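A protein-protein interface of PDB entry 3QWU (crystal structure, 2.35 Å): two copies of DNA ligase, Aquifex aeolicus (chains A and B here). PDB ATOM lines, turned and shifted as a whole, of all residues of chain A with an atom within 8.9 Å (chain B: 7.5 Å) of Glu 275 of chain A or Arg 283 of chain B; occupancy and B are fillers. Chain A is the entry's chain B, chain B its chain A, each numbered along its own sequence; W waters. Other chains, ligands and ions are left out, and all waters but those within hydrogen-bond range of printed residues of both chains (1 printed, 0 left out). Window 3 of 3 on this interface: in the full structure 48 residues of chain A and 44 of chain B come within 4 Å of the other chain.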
ATOM      1  N   ILE A 259      -7.348  34.584 -10.431  1.00  0.00           N
ATOM      2  CA  ILE A 259      -7.499  33.709  -9.269  1.00  0.00           C
ATOM      3  C   ILE A 259      -8.864  33.876  -8.648  1.00  0.00           C
ATOM      4  O   ILE A 259      -9.546  32.903  -8.312  1.00  0.00           O
ATOM      5  CB  ILE A 259      -6.416  33.933  -8.195  1.00  0.00           C
ATOM      6  CG1 ILE A 259      -5.039  33.550  -8.753  1.00  0.00           C
ATOM      7  CG2 ILE A 259      -6.666  33.024  -6.965  1.00  0.00           C
ATOM      8  CD1 ILE A 259      -3.944  33.879  -7.768  1.00  0.00           C
ATOM      9  N   VAL A 263     -11.718  31.287  -7.797  1.00  0.00           N
ATOM     10  CA  VAL A 263     -12.233  31.192  -6.438  1.00  0.00           C
ATOM     11  C   VAL A 263     -13.737  31.529  -6.321  1.00  0.00           C
ATOM     12  O   VAL A 263     -14.439  30.896  -5.554  1.00  0.00           O
ATOM     13  CB  VAL A 263     -11.428  32.083  -5.416  1.00  0.00           C
ATOM     14  CG1 VAL A 263     -12.037  31.958  -3.975  1.00  0.00           C
ATOM     15  CG2 VAL A 263      -9.911  31.702  -5.377  1.00  0.00           C
ATOM     16  N   PHE A 265     -16.063  31.148  -8.698  1.00  0.00           N
ATOM     17  CA  PHE A 265     -16.748  29.977  -9.265  1.00  0.00           C
ATOM     18  C   PHE A 265     -16.810  28.829  -8.258  1.00  0.00           C
ATOM     19  O   PHE A 265     -17.815  28.135  -8.152  1.00  0.00           O
ATOM     20  CB  PHE A 265     -16.026  29.546 -10.543  1.00  0.00           C
ATOM     21  CG  PHE A 265     -16.526  28.255 -11.139  1.00  0.00           C
ATOM     22  CD1 PHE A 265     -17.743  28.190 -11.771  1.00  0.00           C
ATOM     23  CD2 PHE A 265     -15.737  27.085 -11.077  1.00  0.00           C
ATOM     24  CE1 PHE A 265     -18.182  26.959 -12.358  1.00  0.00           C
ATOM     25  CE2 PHE A 265     -16.167  25.876 -11.673  1.00  0.00           C
ATOM     26  CZ  PHE A 265     -17.369  25.807 -12.309  1.00  0.00           C
ATOM     27  N   MET A 266     -15.752  28.670  -7.481  1.00  0.00           N
ATOM     28  CA  MET A 266     -15.681  27.572  -6.534  1.00  0.00           C
ATOM     29  C   MET A 266     -16.635  27.866  -5.410  1.00  0.00           C
ATOM     30  O   MET A 266     -17.310  26.956  -4.909  1.00  0.00           O
ATOM     31  CB  MET A 266     -14.269  27.355  -6.029  1.00  0.00           C
ATOM     32  CG  MET A 266     -13.338  26.868  -7.089  1.00  0.00           C
ATOM     33  SD  MET A 266     -11.622  26.655  -6.536  1.00  0.00           S
ATOM     34  CE  MET A 266     -11.841  25.190  -5.551  1.00  0.00           C
ATOM     35  N   GLU A 269     -20.289  27.341  -6.942  1.00  0.00           N
ATOM     36  CA  GLU A 269     -20.673  25.933  -7.150  1.00  0.00           C
ATOM     37  C   GLU A 269     -20.401  24.990  -5.998  1.00  0.00           C
ATOM     38  O   GLU A 269     -20.850  23.815  -6.032  1.00  0.00           O
ATOM     39  CB  GLU A 269     -19.945  25.352  -8.369  1.00  0.00           C
ATOM     40  CG  GLU A 269     -20.312  26.020  -9.657  1.00  0.00           C
ATOM     41  CD  GLU A 269     -21.801  26.026  -9.922  1.00  0.00           C
ATOM     42  OE1 GLU A 269     -22.384  24.941  -9.998  1.00  0.00           O
ATOM     43  OE2 GLU A 269     -22.396  27.111 -10.069  1.00  0.00           O
ATOM     44  N   GLY A 270     -19.611  25.449  -5.020  1.00  0.00           N
ATOM     45  CA  GLY A 270     -19.262  24.608  -3.877  1.00  0.00           C
ATOM     46  C   GLY A 270     -17.939  23.890  -4.065  1.00  0.00           C
ATOM     47  O   GLY A 270     -17.576  23.427  -5.152  1.00  0.00           O
ATOM     48  N   LEU A 271     -17.187  23.875  -2.988  1.00  0.00           N
ATOM     49  CA  LEU A 271     -15.951  23.158  -2.878  1.00  0.00           C
ATOM     50  C   LEU A 271     -16.015  21.684  -3.275  1.00  0.00           C
ATOM     51  O   LEU A 271     -15.059  21.172  -3.867  1.00  0.00           O
ATOM     52  CB  LEU A 271     -15.452  23.260  -1.425  1.00  0.00           C
ATOM     53  CG  LEU A 271     -14.221  24.109  -1.098  1.00  0.00           C
ATOM     54  CD1 LEU A 271     -14.141  25.355  -1.873  1.00  0.00           C
ATOM     55  CD2 LEU A 271     -14.108  24.382   0.446  1.00  0.00           C
ATOM     56  N   LYS A 272     -17.085  20.982  -2.910  1.00  0.00           N
ATOM     57  CA  LYS A 272     -17.156  19.529  -3.195  1.00  0.00           C
ATOM     58  C   LYS A 272     -17.066  19.225  -4.697  1.00  0.00           C
ATOM     59  O   LYS A 272     -16.383  18.293  -5.128  1.00  0.00           O
ATOM     60  CB  LYS A 272     -18.430  18.874  -2.605  1.00  0.00           C
ATOM     61  CG  LYS A 272     -18.666  17.421  -3.148  1.00  0.00           C
ATOM     62  CD  LYS A 272     -19.145  16.405  -2.122  1.00  0.00           C
ATOM     63  CE  LYS A 272     -18.960  14.991  -2.667  1.00  0.00           C
ATOM     64  NZ  LYS A 272     -17.507  14.676  -2.970  1.00  0.00           N
ATOM     65  N   THR A 273     -17.724  20.041  -5.498  1.00  0.00           N
ATOM     66  CA  THR A 273     -17.772  19.794  -6.922  1.00  0.00           C
ATOM     67  C   THR A 273     -16.574  20.453  -7.644  1.00  0.00           C
ATOM     68  O   THR A 273     -16.417  20.294  -8.860  1.00  0.00           O
ATOM     69  CB  THR A 273     -19.163  20.209  -7.478  1.00  0.00           C
ATOM     70  OG1 THR A 273     -19.130  21.529  -8.020  1.00  0.00           O
ATOM     71  CG2 THR A 273     -20.256  20.112  -6.354  1.00  0.00           C
ATOM     72  N   THR A 274     -15.715  21.170  -6.904  1.00  0.00           N
ATOM     73  CA  THR A 274     -14.614  21.912  -7.557  1.00  0.00           C
ATOM     74  C   THR A 274     -13.203  21.677  -6.988  1.00  0.00           C
ATOM     75  O   THR A 274     -12.285  22.414  -7.323  1.00  0.00           O
ATOM     76  CB  THR A 274     -14.903  23.442  -7.640  1.00  0.00           C
ATOM     77  OG1 THR A 274     -15.048  23.992  -6.324  1.00  0.00           O
ATOM     78  CG2 THR A 274     -16.167  23.708  -8.456  1.00  0.00           C
ATOM     79  N   GLU A 275     -13.036  20.619  -6.188  1.00  0.00           N
ATOM     80  CA  GLU A 275     -11.737  20.246  -5.565  1.00  0.00           C
ATOM     81  C   GLU A 275     -10.631  20.188  -6.567  1.00  0.00           C
ATOM     82  O   GLU A 275      -9.535  20.584  -6.273  1.00  0.00           O
ATOM     83  CB  GLU A 275     -11.797  18.855  -4.916  1.00  0.00           C
ATOM     84  CG  GLU A 275     -12.569  18.754  -3.594  1.00  0.00           C
ATOM     85  CD  GLU A 275     -11.874  19.411  -2.366  1.00  0.00           C
ATOM     86  OE1 GLU A 275     -12.564  20.269  -1.722  1.00  0.00           O
ATOM     87  OE2 GLU A 275     -10.687  19.071  -2.010  1.00  0.00           O
ATOM     88  N   HIS A 276     -10.927  19.671  -7.748  1.00  0.00           N
ATOM     89  CA  HIS A 276      -9.936  19.429  -8.797  1.00  0.00           C
ATOM     90  C   HIS A 276      -9.151  20.697  -9.201  1.00  0.00           C
ATOM     91  O   HIS A 276      -8.063  20.591  -9.772  1.00  0.00           O
ATOM     92  CB  HIS A 276     -10.596  18.750 -10.039  1.00  0.00           C
ATOM     93  CG  HIS A 276     -11.650  19.590 -10.716  1.00  0.00           C
ATOM     94  ND1 HIS A 276     -11.406  20.313 -11.872  1.00  0.00           N
ATOM     95  CD2 HIS A 276     -12.948  19.835 -10.393  1.00  0.00           C
ATOM     96  CE1 HIS A 276     -12.504  20.975 -12.222  1.00  0.00           C
ATOM     97  NE2 HIS A 276     -13.452  20.702 -11.344  1.00  0.00           N
ATOM     98  N   LEU A 277      -9.713  21.871  -8.908  1.00  0.00           N
ATOM     99  CA  LEU A 277      -9.138  23.116  -9.326  1.00  0.00           C
ATOM    100  C   LEU A 277      -7.913  23.444  -8.512  1.00  0.00           C
ATOM    101  O   LEU A 277      -7.036  24.166  -8.989  1.00  0.00           O
ATOM    102  CB  LEU A 277     -10.144  24.269  -9.227  1.00  0.00           C
ATOM    103  CG  LEU A 277     -11.202  24.338 -10.323  1.00  0.00           C
ATOM    104  CD1 LEU A 277     -12.101  25.503 -10.108  1.00  0.00           C
ATOM    105  CD2 LEU A 277     -10.510  24.449 -11.653  1.00  0.00           C
ATOM    106  N   TYR A 278      -7.835  22.921  -7.294  1.00  0.00           N
ATOM    107  CA  TYR A 278      -6.626  23.121  -6.534  1.00  0.00           C
ATOM    108  C   TYR A 278      -5.404  22.654  -7.310  1.00  0.00           C
ATOM    109  O   TYR A 278      -4.527  23.424  -7.545  1.00  0.00           O
ATOM    110  CB  TYR A 278      -6.655  22.387  -5.232  1.00  0.00           C
ATOM    111  CG  TYR A 278      -7.639  22.902  -4.250  1.00  0.00           C
ATOM    112  CD1 TYR A 278      -7.538  24.205  -3.710  1.00  0.00           C
ATOM    113  CD2 TYR A 278      -8.630  22.072  -3.764  1.00  0.00           C
ATOM    114  CE1 TYR A 278      -8.458  24.666  -2.778  1.00  0.00           C
ATOM    115  CE2 TYR A 278      -9.544  22.546  -2.823  1.00  0.00           C
ATOM    116  CZ  TYR A 278      -9.438  23.822  -2.327  1.00  0.00           C
ATOM    117  OH  TYR A 278     -10.365  24.197  -1.396  1.00  0.00           O
ATOM    118  N   GLU A 279      -5.327  21.388  -7.690  1.00  0.00           N
ATOM    119  CA  GLU A 279      -4.155  20.912  -8.429  1.00  0.00           C
ATOM    120  C   GLU A 279      -3.970  21.632  -9.783  1.00  0.00           C
ATOM    121  O   GLU A 279      -2.848  21.900 -10.239  1.00  0.00           O
ATOM    122  CB  GLU A 279      -4.213  19.395  -8.637  1.00  0.00           C
ATOM    123  CG  GLU A 279      -3.297  18.902  -9.786  1.00  0.00           C
ATOM    124  CD  GLU A 279      -3.164  17.396  -9.815  1.00  0.00           C
ATOM    125  OE1 GLU A 279      -4.112  16.735  -9.299  1.00  0.00           O
ATOM    126  OE2 GLU A 279      -2.119  16.885 -10.342  1.00  0.00           O
ATOM    127  N   GLU A 280      -5.075  21.951 -10.419  1.00  0.00           N
ATOM    128  CA  GLU A 280      -4.995  22.420 -11.757  1.00  0.00           C
ATOM    129  C   GLU A 280      -4.541  23.857 -11.742  1.00  0.00           C
ATOM    130  O   GLU A 280      -3.853  24.282 -12.625  1.00  0.00           O
ATOM    131  CB  GLU A 280      -6.341  22.257 -12.458  1.00  0.00           C
ATOM    132  CG  GLU A 280      -6.756  20.784 -12.778  1.00  0.00           C
ATOM    133  CD  GLU A 280      -8.255  20.639 -13.039  1.00  0.00           C
ATOM    134  OE1 GLU A 280      -8.929  21.647 -13.394  1.00  0.00           O
ATOM    135  OE2 GLU A 280      -8.788  19.521 -12.853  1.00  0.00           O
ATOM    136  N   LEU A 281      -4.927  24.626 -10.741  1.00  0.00           N
ATOM    137  CA  LEU A 281      -4.352  26.000 -10.587  1.00  0.00           C
ATOM    138  C   LEU A 281      -2.832  25.927 -10.354  1.00  0.00           C
ATOM    139  O   LEU A 281      -2.052  26.738 -10.894  1.00  0.00           O
ATOM    140  CB  LEU A 281      -5.030  26.772  -9.462  1.00  0.00           C
ATOM    141  CG  LEU A 281      -4.455  28.166  -9.145  1.00  0.00           C
ATOM    142  CD1 LEU A 281      -4.420  29.080 -10.320  1.00  0.00           C
ATOM    143  CD2 LEU A 281      -5.202  28.765  -7.931  1.00  0.00           C
ATOM    144  N   GLY A 282      -2.418  24.936  -9.583  1.00  0.00           N
ATOM    145  CA  GLY A 282      -1.010  24.741  -9.287  1.00  0.00           C
ATOM    146  C   GLY A 282      -0.235  24.428 -10.544  1.00  0.00           C
ATOM    147  O   GLY A 282       0.836  25.017 -10.820  1.00  0.00           O
ATOM    148  N   LEU B 237       4.960  28.845   0.465  1.00  0.00           N
ATOM    149  CA  LEU B 237       3.546  28.554   0.396  1.00  0.00           C
ATOM    150  C   LEU B 237       2.699  29.371   1.428  1.00  0.00           C
ATOM    151  O   LEU B 237       1.726  30.013   1.067  1.00  0.00           O
ATOM    152  CB  LEU B 237       3.316  27.063   0.563  1.00  0.00           C
ATOM    153  CG  LEU B 237       3.749  26.239  -0.631  1.00  0.00           C
ATOM    154  CD1 LEU B 237       3.805  24.758  -0.242  1.00  0.00           C
ATOM    155  CD2 LEU B 237       2.838  26.506  -1.823  1.00  0.00           C
ATOM    156  N   ILE B 240       2.064  32.881   0.649  1.00  0.00           N
ATOM    157  CA  ILE B 240       1.054  33.153  -0.347  1.00  0.00           C
ATOM    158  C   ILE B 240      -0.294  33.104   0.347  1.00  0.00           C
ATOM    159  O   ILE B 240      -1.073  34.033   0.254  1.00  0.00           O
ATOM    160  CB  ILE B 240       1.150  32.200  -1.544  1.00  0.00           C
ATOM    161  CG1 ILE B 240       2.489  32.375  -2.218  1.00  0.00           C
ATOM    162  CG2 ILE B 240       0.054  32.517  -2.512  1.00  0.00           C
ATOM    163  CD1 ILE B 240       2.716  31.493  -3.404  1.00  0.00           C
ATOM    164  N   LYS B 241      -0.515  32.061   1.134  1.00  0.00           N
ATOM    165  CA  LYS B 241      -1.797  31.880   1.839  1.00  0.00           C
ATOM    166  C   LYS B 241      -2.153  32.961   2.826  1.00  0.00           C
ATOM    167  O   LYS B 241      -3.294  33.449   2.828  1.00  0.00           O
ATOM    168  CB  LYS B 241      -1.806  30.546   2.580  1.00  0.00           C
ATOM    169  CG  LYS B 241      -2.935  30.349   3.621  1.00  0.00           C
ATOM    170  CD  LYS B 241      -3.978  29.327   3.226  1.00  0.00           C
ATOM    171  CE  LYS B 241      -5.043  29.109   4.318  1.00  0.00           C
ATOM    172  NZ  LYS B 241      -5.291  27.606   4.551  1.00  0.00           N
ATOM    173  N   LEU B 277       3.326  19.624  -4.586  1.00  0.00           N
ATOM    174  CA  LEU B 277       3.368  21.082  -4.576  1.00  0.00           C
ATOM    175  C   LEU B 277       2.322  21.686  -5.540  1.00  0.00           C
ATOM    176  O   LEU B 277       1.888  22.796  -5.355  1.00  0.00           O
ATOM    177  CB  LEU B 277       4.742  21.619  -4.908  1.00  0.00           C
ATOM    178  CG  LEU B 277       5.799  21.774  -3.815  1.00  0.00           C
ATOM    179  CD1 LEU B 277       5.245  22.460  -2.558  1.00  0.00           C
ATOM    180  CD2 LEU B 277       6.432  20.425  -3.461  1.00  0.00           C
ATOM    181  N   TYR B 278       1.879  20.947  -6.530  1.00  0.00           N
ATOM    182  CA  TYR B 278       0.802  21.447  -7.347  1.00  0.00           C
ATOM    183  C   TYR B 278      -0.413  21.783  -6.496  1.00  0.00           C
ATOM    184  O   TYR B 278      -0.863  22.948  -6.443  1.00  0.00           O
ATOM    185  CB  TYR B 278       0.434  20.426  -8.404  1.00  0.00           C
ATOM    186  CG  TYR B 278       1.473  20.225  -9.454  1.00  0.00           C
ATOM    187  CD1 TYR B 278       1.924  21.278 -10.232  1.00  0.00           C
ATOM    188  CD2 TYR B 278       2.019  18.983  -9.679  1.00  0.00           C
ATOM    189  CE1 TYR B 278       2.900  21.087 -11.232  1.00  0.00           C
ATOM    190  CE2 TYR B 278       3.006  18.777 -10.674  1.00  0.00           C
ATOM    191  CZ  TYR B 278       3.422  19.830 -11.450  1.00  0.00           C
ATOM    192  OH  TYR B 278       4.380  19.631 -12.398  1.00  0.00           O
ATOM    193  N   GLU B 279      -0.945  20.771  -5.807  1.00  0.00           N
ATOM    194  CA  GLU B 279      -2.128  20.977  -4.998  1.00  0.00           C
ATOM    195  C   GLU B 279      -1.852  22.007  -3.920  1.00  0.00           C
ATOM    196  O   GLU B 279      -2.669  22.883  -3.655  1.00  0.00           O
ATOM    197  CB  GLU B 279      -2.646  19.661  -4.373  1.00  0.00           C
ATOM    198  CG  GLU B 279      -4.114  19.779  -3.862  1.00  0.00           C
ATOM    199  CD  GLU B 279      -4.552  18.683  -2.887  1.00  0.00           C
ATOM    200  OE1 GLU B 279      -4.291  17.482  -3.160  1.00  0.00           O
ATOM    201  OE2 GLU B 279      -5.188  19.031  -1.855  1.00  0.00           O
ATOM    202  N   GLU B 280      -0.692  21.914  -3.299  1.00  0.00           N
ATOM    203  CA  GLU B 280      -0.363  22.858  -2.253  1.00  0.00           C
ATOM    204  C   GLU B 280      -0.310  24.291  -2.778  1.00  0.00           C
ATOM    205  O   GLU B 280      -0.902  25.202  -2.160  1.00  0.00           O
ATOM    206  CB  GLU B 280       0.911  22.424  -1.527  1.00  0.00           C
ATOM    207  CG  GLU B 280       0.678  21.228  -0.576  1.00  0.00           C
ATOM    208  CD  GLU B 280       1.942  20.333  -0.350  1.00  0.00           C
ATOM    209  OE1 GLU B 280       3.056  20.892  -0.390  1.00  0.00           O
ATOM    210  OE2 GLU B 280       1.819  19.067  -0.123  1.00  0.00           O
ATOM    211  N   LEU B 281       0.308  24.524  -3.938  1.00  0.00           N
ATOM    212  CA  LEU B 281       0.302  25.900  -4.466  1.00  0.00           C
ATOM    213  C   LEU B 281      -1.163  26.429  -4.721  1.00  0.00           C
ATOM    214  O   LEU B 281      -1.473  27.555  -4.391  1.00  0.00           O
ATOM    215  CB  LEU B 281       1.259  26.075  -5.673  1.00  0.00           C
ATOM    216  CG  LEU B 281       1.176  27.484  -6.329  1.00  0.00           C
ATOM    217  CD1 LEU B 281       1.545  28.636  -5.375  1.00  0.00           C
ATOM    218  CD2 LEU B 281       1.992  27.559  -7.637  1.00  0.00           C
ATOM    219  N   GLY B 282      -2.036  25.586  -5.276  1.00  0.00           N
ATOM    220  CA  GLY B 282      -3.441  25.870  -5.486  1.00  0.00           C
ATOM    221  C   GLY B 282      -4.169  26.209  -4.192  1.00  0.00           C
ATOM    222  O   GLY B 282      -4.931  27.182  -4.105  1.00  0.00           O
ATOM    223  N   ARG B 283      -3.933  25.400  -3.165  1.00  0.00           N
ATOM    224  CA  ARG B 283      -4.516  25.651  -1.837  1.00  0.00           C
ATOM    225  C   ARG B 283      -4.033  26.898  -1.232  1.00  0.00           C
ATOM    226  O   ARG B 283      -4.757  27.576  -0.583  1.00  0.00           O
ATOM    227  CB  ARG B 283      -4.217  24.491  -0.885  1.00  0.00           C
ATOM    228  CG  ARG B 283      -5.110  23.318  -1.175  1.00  0.00           C
ATOM    229  CD  ARG B 283      -4.917  22.212  -0.165  1.00  0.00           C
ATOM    230  NE  ARG B 283      -5.930  21.184  -0.386  1.00  0.00           N
ATOM    231  CZ  ARG B 283      -7.211  21.280  -0.025  1.00  0.00           C
ATOM    232  NH1 ARG B 283      -7.694  22.368   0.617  1.00  0.00           N
ATOM    233  NH2 ARG B 283      -8.031  20.266  -0.318  1.00  0.00           N
ATOM    234  N   ALA B 284      -2.777  27.209  -1.393  1.00  0.00           N
ATOM    235  CA  ALA B 284      -2.301  28.429  -0.858  1.00  0.00           C
ATOM    236  C   ALA B 284      -3.131  29.607  -1.416  1.00  0.00           C
ATOM    237  O   ALA B 284      -3.585  30.415  -0.639  1.00  0.00           O
ATOM    238  CB  ALA B 284      -0.853  28.575  -1.141  1.00  0.00           C
ATOM    239  N   PHE B 285      -3.349  29.707  -2.729  1.00  0.00           N
ATOM    240  CA  PHE B 285      -4.136  30.815  -3.260  1.00  0.00           C
ATOM    241  C   PHE B 285      -5.609  30.640  -2.970  1.00  0.00           C
ATOM    242  O   PHE B 285      -6.293  31.558  -2.551  1.00  0.00           O
ATOM    243  CB  PHE B 285      -4.015  30.925  -4.761  1.00  0.00           C
ATOM    244  CG  PHE B 285      -2.704  31.491  -5.245  1.00  0.00           C
ATOM    245  CD1 PHE B 285      -2.422  32.848  -5.118  1.00  0.00           C
ATOM    246  CD2 PHE B 285      -1.798  30.704  -5.875  1.00  0.00           C
ATOM    247  CE1 PHE B 285      -1.254  33.371  -5.580  1.00  0.00           C
ATOM    248  CE2 PHE B 285      -0.609  31.245  -6.301  1.00  0.00           C
ATOM    249  CZ  PHE B 285      -0.367  32.589  -6.171  1.00  0.00           C
ATOM    250  N   ILE B 286      -6.129  29.462  -3.228  1.00  0.00           N
ATOM    251  CA  ILE B 286      -7.549  29.292  -3.161  1.00  0.00           C
ATOM    252  C   ILE B 286      -8.054  29.330  -1.715  1.00  0.00           C
ATOM    253  O   ILE B 286      -9.052  29.995  -1.433  1.00  0.00           O
ATOM    254  CB  ILE B 286      -7.989  27.987  -3.804  1.00  0.00           C
ATOM    255  CG1 ILE B 286      -7.701  28.017  -5.316  1.00  0.00           C
ATOM    256  CG2 ILE B 286      -9.468  27.772  -3.503  1.00  0.00           C
ATOM    257  CD1 ILE B 286      -8.044  26.700  -6.110  1.00  0.00           C
ATOM    258  N   ASP B 287      -7.429  28.613  -0.793  1.00  0.00           N
ATOM    259  CA  ASP B 287      -7.999  28.615   0.565  1.00  0.00           C
ATOM    260  C   ASP B 287      -7.843  29.915   1.333  1.00  0.00           C
ATOM    261  O   ASP B 287      -8.710  30.249   2.129  1.00  0.00           O
ATOM    262  CB  ASP B 287      -7.469  27.482   1.389  1.00  0.00           C
ATOM    263  CG  ASP B 287      -7.908  26.181   0.880  1.00  0.00           C
ATOM    264  OD1 ASP B 287      -8.994  26.115   0.233  1.00  0.00           O
ATOM    265  OD2 ASP B 287      -7.150  25.227   1.089  1.00  0.00           O
ATOM    266  N   GLY B 288      -6.803  30.687   1.079  1.00  0.00           N
ATOM    267  CA  GLY B 288      -6.696  31.998   1.733  1.00  0.00           C
ATOM    268  C   GLY B 288      -7.792  32.945   1.300  1.00  0.00           C
ATOM    269  O   GLY B 288      -8.348  33.655   2.084  1.00  0.00           O
ATOM    270  N   LEU B 289      -8.114  32.908   0.030  1.00  0.00           N
ATOM    271  CA  LEU B 289      -9.138  33.766  -0.542  1.00  0.00           C
ATOM    272  C   LEU B 289     -10.514  33.260  -0.134  1.00  0.00           C
ATOM    273  O   LEU B 289     -11.364  34.054   0.184  1.00  0.00           O
ATOM    274  CB  LEU B 289      -8.971  33.841  -2.088  1.00  0.00           C
ATOM    275  CG  LEU B 289      -8.717  35.164  -2.817  1.00  0.00           C
ATOM    276  CD1 LEU B 289      -8.239  36.354  -1.936  1.00  0.00           C
ATOM    277  CD2 LEU B 289      -7.791  34.981  -3.988  1.00  0.00           C
ATOM    278  N   PHE B 290     -10.719  31.940  -0.115  1.00  0.00           N
ATOM    279  CA  PHE B 290     -12.009  31.355   0.319  1.00  0.00           C
ATOM    280  C   PHE B 290     -12.324  31.768   1.730  1.00  0.00           C
ATOM    281  O   PHE B 290     -13.441  32.114   2.039  1.00  0.00           O
ATOM    282  CB  PHE B 290     -11.987  29.815   0.283  1.00  0.00           C
ATOM    283  CG  PHE B 290     -13.257  29.224  -0.101  1.00  0.00           C
ATOM    284  CD1 PHE B 290     -13.579  29.082  -1.445  1.00  0.00           C
ATOM    285  CD2 PHE B 290     -14.165  28.815   0.850  1.00  0.00           C
ATOM    286  CE1 PHE B 290     -14.827  28.558  -1.857  1.00  0.00           C
ATOM    287  CE2 PHE B 290     -15.424  28.257   0.474  1.00  0.00           C
ATOM    288  CZ  PHE B 290     -15.747  28.134  -0.885  1.00  0.00           C
ATOM    289  N   GLN B 291     -11.324  31.721   2.603  1.00  0.00           N
ATOM    290  CA  GLN B 291     -11.509  32.205   3.957  1.00  0.00           C
ATOM    291  C   GLN B 291     -11.799  33.670   4.046  1.00  0.00           C
ATOM    292  O   GLN B 291     -12.471  34.086   4.974  1.00  0.00           O
ATOM    293  CB  GLN B 291     -10.251  31.990   4.774  1.00  0.00           C
ATOM    294  CG  GLN B 291      -9.994  30.580   5.188  1.00  0.00           C
ATOM    295  CD  GLN B 291      -8.570  30.424   5.711  1.00  0.00           C
ATOM    296  OE1 GLN B 291      -7.987  29.362   5.586  1.00  0.00           O
ATOM    297  NE2 GLN B 291      -8.017  31.490   6.298  1.00  0.00           N
HETATM  298  O   HOH W   1     -10.844  21.856   0.302  1.00  0.00           O
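OD1 of Asp 287 of chain B is in hydrogen-bond range of OH of Tyr 278 of chain A, at 2.9 Å. The guanidinium group (NH2) of Arg 283 of chain B is in salt-bridge range of the side-chain carboxylate (OE2) of Glu 275 of chain A.
The guanidinium group (NE) of Arg 283 of chain B lies within salt-bridge range of the side-chain carboxylate (OE2) of Glu 279 of chain B. OD2 of Asp 287 of chain B lies within salt-bridge range of NH1 of Arg 283 of chain B.
Among the printed residues, merely in contact across the chains: Ile 259 of chain A with Phe 285 of chain B, Ile 259 of chain A with Leu 289 of chain B, Met 266 of chain A with Ile 286 of chain B, Leu 271 of chain A with Phe 290 of chain B, Leu 277 of chain A with Ile 286 of chain B, Tyr 278 of chain A with Tyr 278 of chain B, Tyr 278 of chain A with Glu 279 of chain B, Tyr 278 of chain A with Gly 282 of chain B, Tyr 278 of chain A with Arg 283 of chain B, Tyr 278 of chain A with Ile 286 of chain B, Glu 279 of chain A with Glu 279 of chain B, Leu 281 of chain A with Ile 286 of chain B and Gly 282 of chain A with Tyr 278 of chain B.
Printed residues of chain B within 4 Å of Met 266 of chain A: Ile 286. Glu 275 of chain A touches just one residue of chain B: Arg 283. Printed residues of chain B within 4 Å of Glu 279 of chain A: Glu 279. Of the printed residues of chain A, Glu 279 of chain B touches Tyr 278 and Glu 279. Of chain A, only Glu 275 (3.4 Å) and Tyr 278 (3.6 Å) come within 4 Å of Arg 283 of chain B. Ala 284 of chain B touches none of the printed residues of chain A. The nearest residue of chain B that does not touch Glu 275 of chain A is Glu 279 of chain B (5.5 Å). The nearest residue of chain A that does not touch Arg 283 of chain B is Leu 281 of chain A (6.0 Å). The nearest printed residue of chain B that does not touch Leu 277 of chain A is Gly 282 of chain B (5.3 Å).
Of the 18 printed residues of chain A, 9 touch a printed residue of chain B. Printed residues of chain A that touch a printed residue of chain B: Ile 259, Met 266, Leu 271, Glu 275, Leu 277, Tyr 278, Glu 279, Leu 281 and Gly 282. Hydrophobic or aromatic side chains of chain A that line the printed part of chain B: Ile 259, Met 266, Leu 271, Tyr 278 and Leu 281. Of the 18 printed residues of chain B, 9 touch a printed residue of chain A.
Tyr 278 of chain B touches its own counterpart, Tyr 278 of chain A. Tyr 278 of chain A touches Glu 279 of chain B, but with the chains exchanged Glu 279 of chain A does not touch Tyr 278 of chain B (4.04 Å). Tyr 278 of chain A touches Gly 282 of chain B, and with the chains exchanged Gly 282 of chain A touches Tyr 278 of chain B. Glu 279 of chain B touches its own counterpart, Glu 279 of chain A. 6 positions are printed for both chains.
Water W1 lies within hydrogen-bond range of OH of Tyr 278 of chain A (2.9 Å), OE1 of Glu 275 of chain A (3.1 Å) and NH1 of Arg 283 of chain B (3.2 Å).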
